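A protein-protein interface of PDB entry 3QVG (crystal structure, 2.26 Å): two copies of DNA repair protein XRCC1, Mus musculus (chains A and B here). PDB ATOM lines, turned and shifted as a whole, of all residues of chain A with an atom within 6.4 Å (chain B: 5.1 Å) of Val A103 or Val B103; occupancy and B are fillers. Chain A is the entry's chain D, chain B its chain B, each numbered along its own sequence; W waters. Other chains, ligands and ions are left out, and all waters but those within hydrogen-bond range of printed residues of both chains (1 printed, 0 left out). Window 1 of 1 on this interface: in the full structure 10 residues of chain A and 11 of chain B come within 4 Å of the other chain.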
ATOM      1  N   GLU A  62       3.715 -11.425  21.630  1.00  0.00           N
ATOM      2  CA  GLU A  62       4.109 -10.948  20.313  1.00  0.00           C
ATOM      3  C   GLU A  62       3.539  -9.553  20.081  1.00  0.00           C
ATOM      4  O   GLU A  62       2.793  -9.037  20.913  1.00  0.00           O
ATOM      5  CB  GLU A  62       3.617 -11.913  19.236  1.00  0.00           C
ATOM      6  CG  GLU A  62       2.142 -12.244  19.349  1.00  0.00           C
ATOM      7  CD  GLU A  62       1.739 -13.405  18.466  1.00  0.00           C
ATOM      8  OE1 GLU A  62       2.638 -14.138  18.001  1.00  0.00           O
ATOM      9  OE2 GLU A  62       0.524 -13.584  18.240  1.00  0.00           O
ATOM     10  N   TRP A  63       3.896  -8.943  18.954  1.00  0.00           N
ATOM     11  CA  TRP A  63       3.393  -7.616  18.615  1.00  0.00           C
ATOM     12  C   TRP A  63       1.877  -7.563  18.743  1.00  0.00           C
ATOM     13  O   TRP A  63       1.181  -8.515  18.390  1.00  0.00           O
ATOM     14  CB  TRP A  63       3.803  -7.224  17.196  1.00  0.00           C
ATOM     15  CG  TRP A  63       3.348  -5.850  16.821  1.00  0.00           C
ATOM     16  CD1 TRP A  63       2.160  -5.509  16.239  1.00  0.00           C
ATOM     17  CD2 TRP A  63       4.066  -4.625  17.014  1.00  0.00           C
ATOM     18  NE1 TRP A  63       2.097  -4.149  16.053  1.00  0.00           N
ATOM     19  CE2 TRP A  63       3.255  -3.582  16.521  1.00  0.00           C
ATOM     20  CE3 TRP A  63       5.317  -4.309  17.553  1.00  0.00           C
ATOM     21  CZ2 TRP A  63       3.654  -2.249  16.550  1.00  0.00           C
ATOM     22  CZ3 TRP A  63       5.712  -2.985  17.582  1.00  0.00           C
ATOM     23  CH2 TRP A  63       4.884  -1.971  17.085  1.00  0.00           C
ATOM     24  N   PHE A  79       9.602  -1.017  21.878  1.00  0.00           N
ATOM     25  CA  PHE A  79       9.004  -2.262  22.331  1.00  0.00           C
ATOM     26  C   PHE A  79      10.075  -3.344  22.422  1.00  0.00           C
ATOM     27  O   PHE A  79      10.744  -3.653  21.434  1.00  0.00           O
ATOM     28  CB  PHE A  79       7.877  -2.672  21.380  1.00  0.00           C
ATOM     29  CG  PHE A  79       6.820  -1.615  21.210  1.00  0.00           C
ATOM     30  CD1 PHE A  79       6.948  -0.638  20.239  1.00  0.00           C
ATOM     31  CD2 PHE A  79       5.704  -1.593  22.030  1.00  0.00           C
ATOM     32  CE1 PHE A  79       5.979   0.337  20.083  1.00  0.00           C
ATOM     33  CE2 PHE A  79       4.730  -0.621  21.881  1.00  0.00           C
ATOM     34  CZ  PHE A  79       4.869   0.346  20.908  1.00  0.00           C
ATOM     35  N   ARG A  81      11.730  -7.087  24.604  1.00  0.00           N
ATOM     36  CA  ARG A  81      11.447  -8.321  25.330  1.00  0.00           C
ATOM     37  C   ARG A  81      12.142  -8.358  26.688  1.00  0.00           C
ATOM     38  O   ARG A  81      13.181  -7.732  26.876  1.00  0.00           O
ATOM     39  CB  ARG A  81      11.863  -9.537  24.504  1.00  0.00           C
ATOM     40  CG  ARG A  81      11.124  -9.658  23.194  1.00  0.00           C
ATOM     41  CD  ARG A  81      11.241 -11.052  22.619  1.00  0.00           C
ATOM     42  NE  ARG A  81      10.458 -11.182  21.395  1.00  0.00           N
ATOM     43  CZ  ARG A  81       9.129 -11.180  21.359  1.00  0.00           C
ATOM     44  NH1 ARG A  81       8.431 -11.050  22.481  1.00  0.00           N
ATOM     45  NH2 ARG A  81       8.497 -11.303  20.200  1.00  0.00           N
ATOM     46  N   HIS A  97      18.563  -1.729  23.354  1.00  0.00           N
ATOM     47  CA  HIS A  97      17.269  -2.402  23.308  1.00  0.00           C
ATOM     48  C   HIS A  97      16.968  -3.001  21.932  1.00  0.00           C
ATOM     49  O   HIS A  97      16.224  -3.973  21.829  1.00  0.00           O
ATOM     50  CB  HIS A  97      16.152  -1.443  23.713  1.00  0.00           C
ATOM     51  CG  HIS A  97      15.911  -0.346  22.723  1.00  0.00           C
ATOM     52  ND1 HIS A  97      15.178  -0.533  21.571  1.00  0.00           N
ATOM     53  CD2 HIS A  97      16.308   0.947  22.713  1.00  0.00           C
ATOM     54  CE1 HIS A  97      15.130   0.600  20.894  1.00  0.00           C
ATOM     55  NE2 HIS A  97      15.808   1.516  21.565  1.00  0.00           N
ATOM     56  N   GLN A  98      17.548  -2.425  20.881  1.00  0.00           N
ATOM     57  CA  GLN A  98      17.315  -2.912  19.519  1.00  0.00           C
ATOM     58  C   GLN A  98      17.579  -4.407  19.365  1.00  0.00           C
ATOM     59  O   GLN A  98      16.983  -5.068  18.513  1.00  0.00           O
ATOM     60  CB  GLN A  98      18.163  -2.139  18.506  1.00  0.00           C
ATOM     61  CG  GLN A  98      17.740  -0.694  18.307  1.00  0.00           C
ATOM     62  CD  GLN A  98      18.376   0.235  19.311  1.00  0.00           C
ATOM     63  OE1 GLN A  98      18.862  -0.198  20.354  1.00  0.00           O
ATOM     64  NE2 GLN A  98      18.390   1.525  18.998  1.00  0.00           N
ATOM     65  N   LEU A  99      18.481  -4.931  20.187  1.00  0.00           N
ATOM     66  CA  LEU A  99      18.866  -6.332  20.116  1.00  0.00           C
ATOM     67  C   LEU A  99      17.767  -7.255  20.636  1.00  0.00           C
ATOM     68  O   LEU A  99      17.853  -8.475  20.492  1.00  0.00           O
ATOM     69  CB  LEU A  99      20.157  -6.562  20.903  1.00  0.00           C
ATOM     70  CG  LEU A  99      21.401  -5.831  20.395  1.00  0.00           C
ATOM     71  CD1 LEU A  99      22.542  -5.955  21.393  1.00  0.00           C
ATOM     72  CD2 LEU A  99      21.815  -6.365  19.036  1.00  0.00           C
ATOM     73  N   TYR A 100      16.734  -6.674  21.238  1.00  0.00           N
ATOM     74  CA  TYR A 100      15.657  -7.462  21.828  1.00  0.00           C
ATOM     75  C   TYR A 100      14.301  -6.880  21.455  1.00  0.00           C
ATOM     76  O   TYR A 100      13.300  -7.122  22.130  1.00  0.00           O
ATOM     77  CB  TYR A 100      15.802  -7.493  23.348  1.00  0.00           C
ATOM     78  CG  TYR A 100      17.217  -7.745  23.817  1.00  0.00           C
ATOM     79  CD1 TYR A 100      17.684  -9.037  24.017  1.00  0.00           C
ATOM     80  CD2 TYR A 100      18.087  -6.688  24.057  1.00  0.00           C
ATOM     81  CE1 TYR A 100      18.980  -9.272  24.444  1.00  0.00           C
ATOM     82  CE2 TYR A 100      19.384  -6.912  24.487  1.00  0.00           C
ATOM     83  CZ  TYR A 100      19.825  -8.206  24.678  1.00  0.00           C
ATOM     84  OH  TYR A 100      21.117  -8.437  25.102  1.00  0.00           O
ATOM     85  N   GLY A 101      14.278  -6.110  20.375  1.00  0.00           N
ATOM     86  CA  GLY A 101      13.075  -5.414  19.963  1.00  0.00           C
ATOM     87  C   GLY A 101      11.938  -6.331  19.562  1.00  0.00           C
ATOM     88  O   GLY A 101      12.144  -7.491  19.210  1.00  0.00           O
ATOM     89  N   VAL A 102      10.724  -5.798  19.619  1.00  0.00           N
ATOM     90  CA  VAL A 102       9.551  -6.534  19.186  1.00  0.00           C
ATOM     91  C   VAL A 102       8.909  -5.803  18.014  1.00  0.00           C
ATOM     92  O   VAL A 102       8.593  -4.617  18.108  1.00  0.00           O
ATOM     93  CB  VAL A 102       8.532  -6.687  20.330  1.00  0.00           C
ATOM     94  CG1 VAL A 102       7.353  -7.540  19.883  1.00  0.00           C
ATOM     95  CG2 VAL A 102       9.204  -7.294  21.552  1.00  0.00           C
ATOM     96  N   VAL A 103       8.732  -6.518  16.907  1.00  0.00           N
ATOM     97  CA  VAL A 103       8.175  -5.938  15.695  1.00  0.00           C
ATOM     98  C   VAL A 103       7.030  -6.799  15.167  1.00  0.00           C
ATOM     99  O   VAL A 103       6.940  -7.984  15.489  1.00  0.00           O
ATOM    100  CB  VAL A 103       9.255  -5.800  14.605  1.00  0.00           C
ATOM    101  CG1 VAL A 103      10.398  -4.917  15.097  1.00  0.00           C
ATOM    102  CG2 VAL A 103       9.768  -7.174  14.187  1.00  0.00           C
ATOM    103  N   PRO A 104       6.141  -6.200  14.357  1.00  0.00           N
ATOM    104  CA  PRO A 104       5.012  -6.927  13.768  1.00  0.00           C
ATOM    105  C   PRO A 104       5.475  -8.047  12.843  1.00  0.00           C
ATOM    106  O   PRO A 104       6.568  -7.980  12.277  1.00  0.00           O
ATOM    107  CB  PRO A 104       4.292  -5.850  12.950  1.00  0.00           C
ATOM    108  CG  PRO A 104       4.705  -4.558  13.566  1.00  0.00           C
ATOM    109  CD  PRO A 104       6.117  -4.770  14.006  1.00  0.00           C
ATOM    110  N   GLN A 105       4.636  -9.066  12.692  1.00  0.00           N
ATOM    111  CA  GLN A 105       4.933 -10.183  11.808  1.00  0.00           C
ATOM    112  C   GLN A 105       4.374  -9.938  10.407  1.00  0.00           C
ATOM    113  O   GLN A 105       3.159  -9.960  10.203  1.00  0.00           O
ATOM    114  CB  GLN A 105       4.358 -11.480  12.380  1.00  0.00           C
ATOM    115  CG  GLN A 105       4.523 -12.680  11.463  1.00  0.00           C
ATOM    116  CD  GLN A 105       5.975 -12.968  11.144  1.00  0.00           C
ATOM    117  OE1 GLN A 105       6.838 -12.897  12.019  1.00  0.00           O
ATOM    118  NE2 GLN A 105       6.256 -13.283   9.883  1.00  0.00           N
ATOM    119  N   TRP B  63      18.782  -9.542  10.300  1.00  0.00           N
ATOM    120  CA  TRP B  63      19.707  -8.943  11.257  1.00  0.00           C
ATOM    121  C   TRP B  63      21.153  -9.351  10.989  1.00  0.00           C
ATOM    122  O   TRP B  63      21.419 -10.467  10.546  1.00  0.00           O
ATOM    123  CB  TRP B  63      19.318  -9.304  12.689  1.00  0.00           C
ATOM    124  CG  TRP B  63      20.100  -8.538  13.702  1.00  0.00           C
ATOM    125  CD1 TRP B  63      21.232  -8.945  14.342  1.00  0.00           C
ATOM    126  CD2 TRP B  63      19.820  -7.217  14.177  1.00  0.00           C
ATOM    127  NE1 TRP B  63      21.668  -7.963  15.197  1.00  0.00           N
ATOM    128  CE2 TRP B  63      20.819  -6.891  15.112  1.00  0.00           C
ATOM    129  CE3 TRP B  63      18.817  -6.282  13.908  1.00  0.00           C
ATOM    130  CZ2 TRP B  63      20.844  -5.671  15.778  1.00  0.00           C
ATOM    131  CZ3 TRP B  63      18.845  -5.072  14.568  1.00  0.00           C
ATOM    132  CH2 TRP B  63      19.851  -4.778  15.493  1.00  0.00           C
ATOM    133  N   GLN B  98       8.570   1.670  13.700  1.00  0.00           N
ATOM    134  CA  GLN B  98       8.524   0.487  14.550  1.00  0.00           C
ATOM    135  C   GLN B  98       7.660  -0.604  13.935  1.00  0.00           C
ATOM    136  O   GLN B  98       7.833  -1.784  14.238  1.00  0.00           O
ATOM    137  CB  GLN B  98       7.994   0.828  15.947  1.00  0.00           C
ATOM    138  CG  GLN B  98       8.900   1.720  16.785  1.00  0.00           C
ATOM    139  CD  GLN B  98       8.631   3.194  16.574  1.00  0.00           C
ATOM    140  OE1 GLN B  98       8.215   3.614  15.494  1.00  0.00           O
ATOM    141  NE2 GLN B  98       8.859   3.992  17.612  1.00  0.00           N
ATOM    142  N   GLY B 101      10.183  -2.525  11.799  1.00  0.00           N
ATOM    143  CA  GLY B 101      11.521  -2.653  12.344  1.00  0.00           C
ATOM    144  C   GLY B 101      12.189  -3.989  12.081  1.00  0.00           C
ATOM    145  O   GLY B 101      11.524  -5.013  11.902  1.00  0.00           O
ATOM    146  N   VAL B 102      13.518  -3.972  12.062  1.00  0.00           N
ATOM    147  CA  VAL B 102      14.308  -5.182  11.891  1.00  0.00           C
ATOM    148  C   VAL B 102      15.057  -5.494  13.183  1.00  0.00           C
ATOM    149  O   VAL B 102      15.802  -4.662  13.700  1.00  0.00           O
ATOM    150  CB  VAL B 102      15.315  -5.040  10.731  1.00  0.00           C
ATOM    151  CG1 VAL B 102      16.198  -6.276  10.631  1.00  0.00           C
ATOM    152  CG2 VAL B 102      14.582  -4.793   9.416  1.00  0.00           C
ATOM    153  N   VAL B 103      14.842  -6.693  13.709  1.00  0.00           N
ATOM    154  CA  VAL B 103      15.496  -7.117  14.940  1.00  0.00           C
ATOM    155  C   VAL B 103      16.092  -8.509  14.776  1.00  0.00           C
ATOM    156  O   VAL B 103      15.742  -9.230  13.842  1.00  0.00           O
ATOM    157  CB  VAL B 103      14.513  -7.127  16.126  1.00  0.00           C
ATOM    158  CG1 VAL B 103      14.033  -5.719  16.438  1.00  0.00           C
ATOM    159  CG2 VAL B 103      13.340  -8.057  15.840  1.00  0.00           C
ATOM    160  N   PRO B 104      17.010  -8.890  15.680  1.00  0.00           N
ATOM    161  CA  PRO B 104      17.546 -10.253  15.674  1.00  0.00           C
ATOM    162  C   PRO B 104      16.420 -11.284  15.639  1.00  0.00           C
ATOM    163  O   PRO B 104      15.418 -11.134  16.338  1.00  0.00           O
ATOM    164  CB  PRO B 104      18.296 -10.330  17.005  1.00  0.00           C
ATOM    165  CG  PRO B 104      18.745  -8.929  17.247  1.00  0.00           C
ATOM    166  CD  PRO B 104      17.636  -8.055  16.722  1.00  0.00           C
ATOM    167  N   GLN B 105      16.580 -12.316  14.819  1.00  0.00           N
ATOM    168  CA  GLN B 105      15.551 -13.337  14.682  1.00  0.00           C
ATOM    169  C   GLN B 105      15.419 -14.149  15.963  1.00  0.00           C
ATOM    170  O   GLN B 105      16.366 -14.807  16.394  1.00  0.00           O
ATOM    171  CB  GLN B 105      15.861 -14.255  13.499  1.00  0.00           C
ATOM    172  CG  GLN B 105      16.099 -13.513  12.192  1.00  0.00           C
ATOM    173  CD  GLN B 105      16.406 -14.445  11.037  1.00  0.00           C
ATOM    174  OE1 GLN B 105      17.289 -14.172  10.225  1.00  0.00           O
ATOM    175  NE2 GLN B 105      15.673 -15.551  10.954  1.00  0.00           N
HETATM  176  O   HOH W   1       9.507  -1.919  17.137  1.00  0.00           O
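Val B103 touches Gln A98.
Gln A98 touches Pro B104 (O to CD, 3.5 Å).
Leu A99 touches Trp B63 (CD2 to CZ2, 3.5 Å).
CG of Pro B104 touches O of Leu A99, 3.4 Å away.
Val B103 touches Gly A101.
Gly B101 touches Val A103.
Val A103 touches Val B103 (CG1 to CG1, 3.96 Å).
Pro A104 touches Gln B98 (CD to O, 3.5 Å).
Printed residues of chain B within 4 Å of Gly A101: Val B103 (3.6 Å).
Val A103 touches just these residues of chain B: Gly B101 (3.4 Å) and Val B103 (3.96 Å).
Printed residues of chain A within 4 Å of Gly B101: Val A103.
Val B103 touches just these residues of chain A: Gln A98 (3.7 Å), Gly A101 (3.6 Å) and Val A103 (3.96 Å).
Printed residues of chain A within 4 Å of Pro B104: Gln A98 and Leu A99.
The nearest residue of chain A that does not touch Val B103 is Val A102 (4.6 Å).
The nearest printed residue of chain B that does not touch Gln A98 is Trp B63 (4.2 Å).
Printed residues of chain A that touch a printed residue of chain B: Gln A98, Leu A99, Gly A101, Val A103 and Pro A104.
Of the 7 printed residues of chain B, 5 touch a printed residue of chain A.
Printed residues of chain B that touch a printed residue of chain A: Trp B63, Gln B98, Gly B101, Val B103 and Pro B104.
Among the printed residues, 8 pairs touch across the chains.
Among the printed residues, no Asp or Glu carboxylate lies within 4 Å of a Lys or Arg side-chain nitrogen of the other chain.
Gln A98 touches Val B103, but with the chains exchanged Val A103 does not touch Gln B98 (4.1 Å).
Gln A98 touches Pro B104, and with the chains exchanged Pro A104 touches Gln B98.
Gly A101 touches Val B103, and with the chains exchanged Val A103 touches Gly B101.
Val B103 touches its own counterpart, Val A103.
Positions printed for both chains: 63, 98, 101, 102, 103, 104 and 105.
Of the 8 pairs that touch across the chains among the printed residues, 5 have their exchanged pair printed and touching as well.
Water W1 bridges the backbone carbonyl oxygen (O) of Val A102 (3.0 Å) and the backbone carbonyl oxygen (O) of Gln B98 (3.4 Å).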
